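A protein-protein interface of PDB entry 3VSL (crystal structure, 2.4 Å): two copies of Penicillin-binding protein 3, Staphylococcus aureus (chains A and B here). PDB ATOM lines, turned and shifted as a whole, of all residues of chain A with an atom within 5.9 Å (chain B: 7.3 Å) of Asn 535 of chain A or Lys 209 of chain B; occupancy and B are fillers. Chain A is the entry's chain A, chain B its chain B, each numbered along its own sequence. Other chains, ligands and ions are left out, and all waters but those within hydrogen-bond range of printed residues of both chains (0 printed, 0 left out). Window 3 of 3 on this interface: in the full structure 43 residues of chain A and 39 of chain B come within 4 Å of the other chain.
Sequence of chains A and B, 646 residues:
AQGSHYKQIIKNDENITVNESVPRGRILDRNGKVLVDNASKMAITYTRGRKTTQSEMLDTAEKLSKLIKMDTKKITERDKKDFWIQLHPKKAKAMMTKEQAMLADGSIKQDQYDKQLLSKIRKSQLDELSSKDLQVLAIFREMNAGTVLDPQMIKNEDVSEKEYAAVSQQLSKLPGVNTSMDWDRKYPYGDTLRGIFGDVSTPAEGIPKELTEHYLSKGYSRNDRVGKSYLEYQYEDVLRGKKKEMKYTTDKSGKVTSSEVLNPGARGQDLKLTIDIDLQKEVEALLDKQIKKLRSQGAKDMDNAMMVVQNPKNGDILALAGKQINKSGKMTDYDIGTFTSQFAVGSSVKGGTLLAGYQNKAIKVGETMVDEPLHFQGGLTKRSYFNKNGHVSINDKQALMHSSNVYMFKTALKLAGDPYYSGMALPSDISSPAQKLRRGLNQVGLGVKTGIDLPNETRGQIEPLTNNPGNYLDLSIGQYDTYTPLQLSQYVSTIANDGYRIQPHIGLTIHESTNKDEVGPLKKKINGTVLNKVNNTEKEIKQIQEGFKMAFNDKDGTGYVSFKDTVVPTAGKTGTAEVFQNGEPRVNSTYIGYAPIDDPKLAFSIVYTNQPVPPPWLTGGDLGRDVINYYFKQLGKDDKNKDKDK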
ATOM      1  N   LEU A 355      15.762 -19.814  15.046  1.00  0.00           N
ATOM      2  CA  LEU A 355      15.107 -18.746  15.804  1.00  0.00           C
ATOM      3  C   LEU A 355      14.061 -17.991  14.961  1.00  0.00           C
ATOM      4  O   LEU A 355      12.900 -17.869  15.351  1.00  0.00           O
ATOM      5  CB  LEU A 355      16.162 -17.771  16.327  1.00  0.00           C
ATOM      6  CG  LEU A 355      16.520 -17.813  17.816  1.00  0.00           C
ATOM      7  CD1 LEU A 355      15.777 -18.909  18.562  1.00  0.00           C
ATOM      8  CD2 LEU A 355      17.999 -17.980  17.968  1.00  0.00           C
ATOM      9  N   GLN A 359       9.883 -18.198  15.744  1.00  0.00           N
ATOM     10  CA  GLN A 359       9.013 -17.073  16.109  1.00  0.00           C
ATOM     11  C   GLN A 359       7.922 -16.833  15.070  1.00  0.00           C
ATOM     12  O   GLN A 359       6.784 -16.470  15.405  1.00  0.00           O
ATOM     13  CB  GLN A 359       9.813 -15.793  16.363  1.00  0.00           C
ATOM     14  CG  GLN A 359      10.829 -15.460  15.303  1.00  0.00           C
ATOM     15  CD  GLN A 359      11.405 -14.077  15.472  1.00  0.00           C
ATOM     16  OE1 GLN A 359      10.688 -13.131  15.813  1.00  0.00           O
ATOM     17  NE2 GLN A 359      12.711 -13.944  15.244  1.00  0.00           N
ATOM     18  N   GLN A 443      17.988  -9.924  14.690  1.00  0.00           N
ATOM     19  CA  GLN A 443      17.776  -9.856  16.118  1.00  0.00           C
ATOM     20  C   GLN A 443      18.999 -10.300  16.882  1.00  0.00           C
ATOM     21  O   GLN A 443      19.260  -9.794  17.981  1.00  0.00           O
ATOM     22  CB  GLN A 443      16.536 -10.645  16.516  1.00  0.00           C
ATOM     23  CG  GLN A 443      15.266  -9.825  16.310  1.00  0.00           C
ATOM     24  CD  GLN A 443      13.996 -10.633  16.521  1.00  0.00           C
ATOM     25  OE1 GLN A 443      14.011 -11.697  17.166  1.00  0.00           O
ATOM     26  NE2 GLN A 443      12.880 -10.129  15.979  1.00  0.00           N
ATOM     27  N   LEU A 531      20.522  -4.245  23.681  1.00  0.00           N
ATOM     28  CA  LEU A 531      19.963  -3.677  22.450  1.00  0.00           C
ATOM     29  C   LEU A 531      18.526  -4.130  22.248  1.00  0.00           C
ATOM     30  O   LEU A 531      17.656  -3.338  21.872  1.00  0.00           O
ATOM     31  CB  LEU A 531      20.802  -4.074  21.246  1.00  0.00           C
ATOM     32  CG  LEU A 531      21.784  -3.014  20.762  1.00  0.00           C
ATOM     33  CD1 LEU A 531      22.353  -2.196  21.914  1.00  0.00           C
ATOM     34  CD2 LEU A 531      22.884  -3.693  19.955  1.00  0.00           C
ATOM     35  N   ASN A 532      18.307  -5.420  22.489  1.00  0.00           N
ATOM     36  CA  ASN A 532      16.995  -6.036  22.468  1.00  0.00           C
ATOM     37  C   ASN A 532      17.150  -7.464  22.976  1.00  0.00           C
ATOM     38  O   ASN A 532      18.280  -7.921  23.203  1.00  0.00           O
ATOM     39  CB  ASN A 532      16.431  -6.038  21.047  1.00  0.00           C
ATOM     40  CG  ASN A 532      17.205  -6.956  20.107  1.00  0.00           C
ATOM     41  OD1 ASN A 532      18.222  -6.553  19.517  1.00  0.00           O
ATOM     42  ND2 ASN A 532      16.710  -8.193  19.939  1.00  0.00           N
ATOM     43  N   LYS A 533      16.031  -8.166  23.158  1.00  0.00           N
ATOM     44  CA  LYS A 533      16.072  -9.608  23.406  1.00  0.00           C
ATOM     45  C   LYS A 533      15.427 -10.295  22.211  1.00  0.00           C
ATOM     46  O   LYS A 533      14.520  -9.740  21.591  1.00  0.00           O
ATOM     47  CB  LYS A 533      15.354  -9.990  24.708  1.00  0.00           C
ATOM     48  CG  LYS A 533      15.359 -11.477  25.039  1.00  0.00           C
ATOM     49  CD  LYS A 533      14.202 -11.799  25.992  1.00  0.00           C
ATOM     50  CE  LYS A 533      14.555 -12.912  26.991  1.00  0.00           C
ATOM     51  NZ  LYS A 533      13.711 -12.888  28.234  1.00  0.00           N
ATOM     52  N   VAL A 534      15.909 -11.479  21.853  1.00  0.00           N
ATOM     53  CA  VAL A 534      15.316 -12.193  20.736  1.00  0.00           C
ATOM     54  C   VAL A 534      13.847 -12.435  21.012  1.00  0.00           C
ATOM     55  O   VAL A 534      13.467 -12.799  22.128  1.00  0.00           O
ATOM     56  CB  VAL A 534      15.995 -13.557  20.479  1.00  0.00           C
ATOM     57  CG1 VAL A 534      17.383 -13.370  19.929  1.00  0.00           C
ATOM     58  CG2 VAL A 534      16.036 -14.398  21.757  1.00  0.00           C
ATOM     59  N   ASN A 535      13.017 -12.231  19.998  1.00  0.00           N
ATOM     60  CA  ASN A 535      11.645 -12.677  20.104  1.00  0.00           C
ATOM     61  C   ASN A 535      11.570 -14.199  20.049  1.00  0.00           C
ATOM     62  O   ASN A 535      11.223 -14.771  19.006  1.00  0.00           O
ATOM     63  CB  ASN A 535      10.797 -12.080  18.998  1.00  0.00           C
ATOM     64  CG  ASN A 535       9.490 -11.616  19.509  1.00  0.00           C
ATOM     65  OD1 ASN A 535       9.383 -11.254  20.680  1.00  0.00           O
ATOM     66  ND2 ASN A 535       8.470 -11.653  18.670  1.00  0.00           N
ATOM     67  N   ASN A 536      11.936 -14.842  21.162  1.00  0.00           N
ATOM     68  CA  ASN A 536      11.855 -16.296  21.307  1.00  0.00           C
ATOM     69  C   ASN A 536      11.760 -16.664  22.789  1.00  0.00           C
ATOM     70  O   ASN A 536      12.236 -15.917  23.646  1.00  0.00           O
ATOM     71  CB  ASN A 536      13.082 -17.001  20.703  1.00  0.00           C
ATOM     72  CG  ASN A 536      13.249 -16.747  19.222  1.00  0.00           C
ATOM     73  OD1 ASN A 536      14.142 -16.004  18.816  1.00  0.00           O
ATOM     74  ND2 ASN A 536      12.403 -17.369  18.405  1.00  0.00           N
ATOM     75  N   THR A 537      11.156 -17.818  23.081  1.00  0.00           N
ATOM     76  CA  THR A 537      11.025 -18.332  24.453  1.00  0.00           C
ATOM     77  C   THR A 537      12.310 -18.983  24.915  1.00  0.00           C
ATOM     78  O   THR A 537      13.089 -19.452  24.083  1.00  0.00           O
ATOM     79  CB  THR A 537       9.927 -19.406  24.540  1.00  0.00           C
ATOM     80  OG1 THR A 537      10.314 -20.552  23.764  1.00  0.00           O
ATOM     81  CG2 THR A 537       8.605 -18.860  24.028  1.00  0.00           C
ATOM     82  N   GLU A 540      12.801 -22.240  23.201  1.00  0.00           N
ATOM     83  CA  GLU A 540      13.339 -22.007  21.862  1.00  0.00           C
ATOM     84  C   GLU A 540      14.829 -21.661  21.931  1.00  0.00           C
ATOM     85  O   GLU A 540      15.642 -22.231  21.205  1.00  0.00           O
ATOM     86  CB  GLU A 540      12.552 -20.907  21.133  1.00  0.00           C
ATOM     87  CG  GLU A 540      11.223 -21.380  20.534  1.00  0.00           C
ATOM     88  CD  GLU A 540      10.357 -20.224  20.073  1.00  0.00           C
ATOM     89  OE1 GLU A 540       9.210 -20.454  19.604  1.00  0.00           O
ATOM     90  OE2 GLU A 540      10.829 -19.076  20.182  1.00  0.00           O
ATOM     91  N   GLU B 205       3.151  -4.374  15.786  1.00  0.00           N
ATOM     92  CA  GLU B 205       4.519  -4.433  16.259  1.00  0.00           C
ATOM     93  C   GLU B 205       4.987  -3.308  17.191  1.00  0.00           C
ATOM     94  O   GLU B 205       5.961  -3.518  17.919  1.00  0.00           O
ATOM     95  CB  GLU B 205       5.465  -4.512  15.069  1.00  0.00           C
ATOM     96  CG  GLU B 205       5.368  -3.339  14.106  1.00  0.00           C
ATOM     97  CD  GLU B 205       6.298  -3.487  12.890  1.00  0.00           C
ATOM     98  OE1 GLU B 205       5.788  -3.602  11.759  1.00  0.00           O
ATOM     99  OE2 GLU B 205       7.538  -3.466  13.054  1.00  0.00           O
ATOM    100  N   GLY B 206       4.332  -2.137  17.178  1.00  0.00           N
ATOM    101  CA  GLY B 206       4.860  -0.953  17.874  1.00  0.00           C
ATOM    102  C   GLY B 206       6.317  -0.699  17.454  1.00  0.00           C
ATOM    103  O   GLY B 206       6.647  -0.807  16.266  1.00  0.00           O
ATOM    104  N   ILE B 207       7.206  -0.378  18.398  1.00  0.00           N
ATOM    105  CA  ILE B 207       8.641  -0.378  18.070  1.00  0.00           C
ATOM    106  C   ILE B 207       9.116  -1.780  17.703  1.00  0.00           C
ATOM    107  O   ILE B 207       8.956  -2.704  18.500  1.00  0.00           O
ATOM    108  CB  ILE B 207       9.534   0.030  19.248  1.00  0.00           C
ATOM    109  CG1 ILE B 207       9.066   1.333  19.886  1.00  0.00           C
ATOM    110  CG2 ILE B 207      10.989   0.167  18.793  1.00  0.00           C
ATOM    111  CD1 ILE B 207       9.928   1.737  21.074  1.00  0.00           C
ATOM    112  N   PRO B 208       9.767  -1.931  16.529  1.00  0.00           N
ATOM    113  CA  PRO B 208      10.296  -3.247  16.124  1.00  0.00           C
ATOM    114  C   PRO B 208      11.376  -3.729  17.092  1.00  0.00           C
ATOM    115  O   PRO B 208      12.158  -2.902  17.598  1.00  0.00           O
ATOM    116  CB  PRO B 208      10.928  -2.975  14.759  1.00  0.00           C
ATOM    117  CG  PRO B 208      10.318  -1.696  14.296  1.00  0.00           C
ATOM    118  CD  PRO B 208      10.064  -0.891  15.531  1.00  0.00           C
ATOM    119  N   LYS B 209      11.403  -5.035  17.346  1.00  0.00           N
ATOM    120  CA  LYS B 209      12.327  -5.624  18.306  1.00  0.00           C
ATOM    121  C   LYS B 209      13.758  -5.129  18.105  1.00  0.00           C
ATOM    122  O   LYS B 209      14.336  -4.529  19.020  1.00  0.00           O
ATOM    123  CB  LYS B 209      12.262  -7.155  18.248  1.00  0.00           C
ATOM    124  CG  LYS B 209      10.989  -7.757  18.863  1.00  0.00           C
ATOM    125  CD  LYS B 209      11.037  -7.810  20.396  1.00  0.00           C
ATOM    126  CE  LYS B 209       9.626  -7.924  20.974  1.00  0.00           C
ATOM    127  NZ  LYS B 209       8.581  -7.907  19.911  1.00  0.00           N
ATOM    128  N   GLU B 210      14.302  -5.335  16.906  1.00  0.00           N
ATOM    129  CA  GLU B 210      15.666  -4.894  16.576  1.00  0.00           C
ATOM    130  C   GLU B 210      15.954  -3.443  16.941  1.00  0.00           C
ATOM    131  O   GLU B 210      17.094  -3.107  17.227  1.00  0.00           O
ATOM    132  CB  GLU B 210      15.996  -5.129  15.095  1.00  0.00           C
ATOM    133  CG  GLU B 210      14.888  -4.726  14.116  1.00  0.00           C
ATOM    134  CD  GLU B 210      13.886  -5.855  13.827  1.00  0.00           C
ATOM    135  OE1 GLU B 210      13.334  -5.886  12.704  1.00  0.00           O
ATOM    136  OE2 GLU B 210      13.633  -6.702  14.718  1.00  0.00           O
ATOM    137  N   LEU B 211      14.921  -2.601  16.961  1.00  0.00           N
ATOM    138  CA  LEU B 211      15.091  -1.162  17.207  1.00  0.00           C
ATOM    139  C   LEU B 211      14.807  -0.697  18.641  1.00  0.00           C
ATOM    140  O   LEU B 211      14.779   0.514  18.911  1.00  0.00           O
ATOM    141  CB  LEU B 211      14.210  -0.362  16.242  1.00  0.00           C
ATOM    142  CG  LEU B 211      14.650  -0.354  14.785  1.00  0.00           C
ATOM    143  CD1 LEU B 211      13.660   0.451  13.971  1.00  0.00           C
ATOM    144  CD2 LEU B 211      16.068   0.221  14.681  1.00  0.00           C
ATOM    145  N   THR B 212      14.596  -1.652  19.546  1.00  0.00           N
ATOM    146  CA  THR B 212      14.031  -1.353  20.867  1.00  0.00           C
ATOM    147  C   THR B 212      14.722  -0.228  21.628  1.00  0.00           C
ATOM    148  O   THR B 212      14.077   0.739  22.049  1.00  0.00           O
ATOM    149  CB  THR B 212      14.000  -2.585  21.772  1.00  0.00           C
ATOM    150  OG1 THR B 212      13.438  -3.682  21.046  1.00  0.00           O
ATOM    151  CG2 THR B 212      13.178  -2.300  23.030  1.00  0.00           C
ATOM    152  N   GLU B 213      16.028  -0.357  21.808  1.00  0.00           N
ATOM    153  CA  GLU B 213      16.745   0.579  22.654  1.00  0.00           C
ATOM    154  C   GLU B 213      16.881   1.900  21.930  1.00  0.00           C
ATOM    155  O   GLU B 213      16.799   2.963  22.540  1.00  0.00           O
ATOM    156  CB  GLU B 213      18.107   0.021  23.019  1.00  0.00           C
ATOM    157  CG  GLU B 213      18.714   0.716  24.215  1.00  0.00           C
ATOM    158  CD  GLU B 213      19.636   1.833  23.801  1.00  0.00           C
ATOM    159  OE1 GLU B 213      19.983   1.853  22.606  1.00  0.00           O
ATOM    160  OE2 GLU B 213      20.018   2.676  24.652  1.00  0.00           O
ATOM    161  N   HIS B 214      17.057   1.827  20.617  1.00  0.00           N
ATOM    162  CA  HIS B 214      17.182   3.017  19.798  1.00  0.00           C
ATOM    163  C   HIS B 214      16.029   3.961  19.999  1.00  0.00           C
ATOM    164  O   HIS B 214      16.222   5.168  20.043  1.00  0.00           O
ATOM    165  CB  HIS B 214      17.242   2.659  18.328  1.00  0.00           C
ATOM    166  CG  HIS B 214      17.260   3.854  17.432  1.00  0.00           C
ATOM    167  ND1 HIS B 214      16.117   4.385  16.877  1.00  0.00           N
ATOM    168  CD2 HIS B 214      18.285   4.634  17.017  1.00  0.00           C
ATOM    169  CE1 HIS B 214      16.441   5.436  16.143  1.00  0.00           C
ATOM    170  NE2 HIS B 214      17.746   5.605  16.208  1.00  0.00           N
ATOM    171  N   ARG B 222       6.830   1.189  24.062  1.00  0.00           N
ATOM    172  CA  ARG B 222       7.023   0.072  23.142  1.00  0.00           C
ATOM    173  C   ARG B 222       5.830  -0.059  22.184  1.00  0.00           C
ATOM    174  O   ARG B 222       5.953  -0.691  21.139  1.00  0.00           O
ATOM    175  CB  ARG B 222       7.254  -1.228  23.926  1.00  0.00           C
ATOM    176  CG  ARG B 222       7.890  -2.362  23.145  1.00  0.00           C
ATOM    177  CD  ARG B 222       7.594  -3.707  23.809  1.00  0.00           C
ATOM    178  NE  ARG B 222       6.297  -4.260  23.401  1.00  0.00           N
ATOM    179  CZ  ARG B 222       5.631  -5.199  24.070  1.00  0.00           C
ATOM    180  NH1 ARG B 222       4.466  -5.642  23.616  1.00  0.00           N
ATOM    181  NH2 ARG B 222       6.127  -5.690  25.199  1.00  0.00           N
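The backbone carbonyl oxygen of Leu 531 of chain A sits at hydrogen-bond distance from the backbone NH of Glu 213 of chain B (3.4 Å).
No position is printed for both chains.
Of the 7 pairs that touch across the chains among the printed residues, none has its exchanged pair printed and touching as well.
Along chain A the printed residues that touch a printed residue of chain B span positions 443 to 535.
Among the printed residues, 7 pairs touch across the chains.
Of the printed residues of chain B, Gln 443 of chain A touches Lys 209 and Glu 210.
Printed residues of chain B within 4 Å of Leu 531 of chain A: Thr 212 and Glu 213.
Asn 535 of chain A touches just one residue of chain B: Lys 209.
Of the printed residues of chain A, Glu 210 of chain B touches Gln 443.
The nearest residue of chain A that does not touch Lys 209 of chain B is Lys 533 of chain A (4.2 Å).
NE2 of Gln 359 of chain A lies within hydrogen-bond range of OE1 of Gln 443 of chain A (3.2 Å).
The side-chain amide oxygen of Gln 443 of chain A is in hydrogen-bond range of the backbone NH of Asn 535 of chain A, at 3.0 Å.
Gln 443 of chain A touches Lys 209 of chain B (NE2 to CB, 3.8 Å).
Gln 443 of chain A touches Glu 210 of chain B.
O of Leu 531 of chain A touches CB of Thr 212 of chain B, at 3.7 Å.
Asn 532 of chain A touches Lys 209 of chain B (CB to O, 3.3 Å).
Asn 532 of chain A touches Thr 212 of chain B.
CE of Lys 209 of chain B touches OD1 of Asn 535 of chain A, at 3.4 Å.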
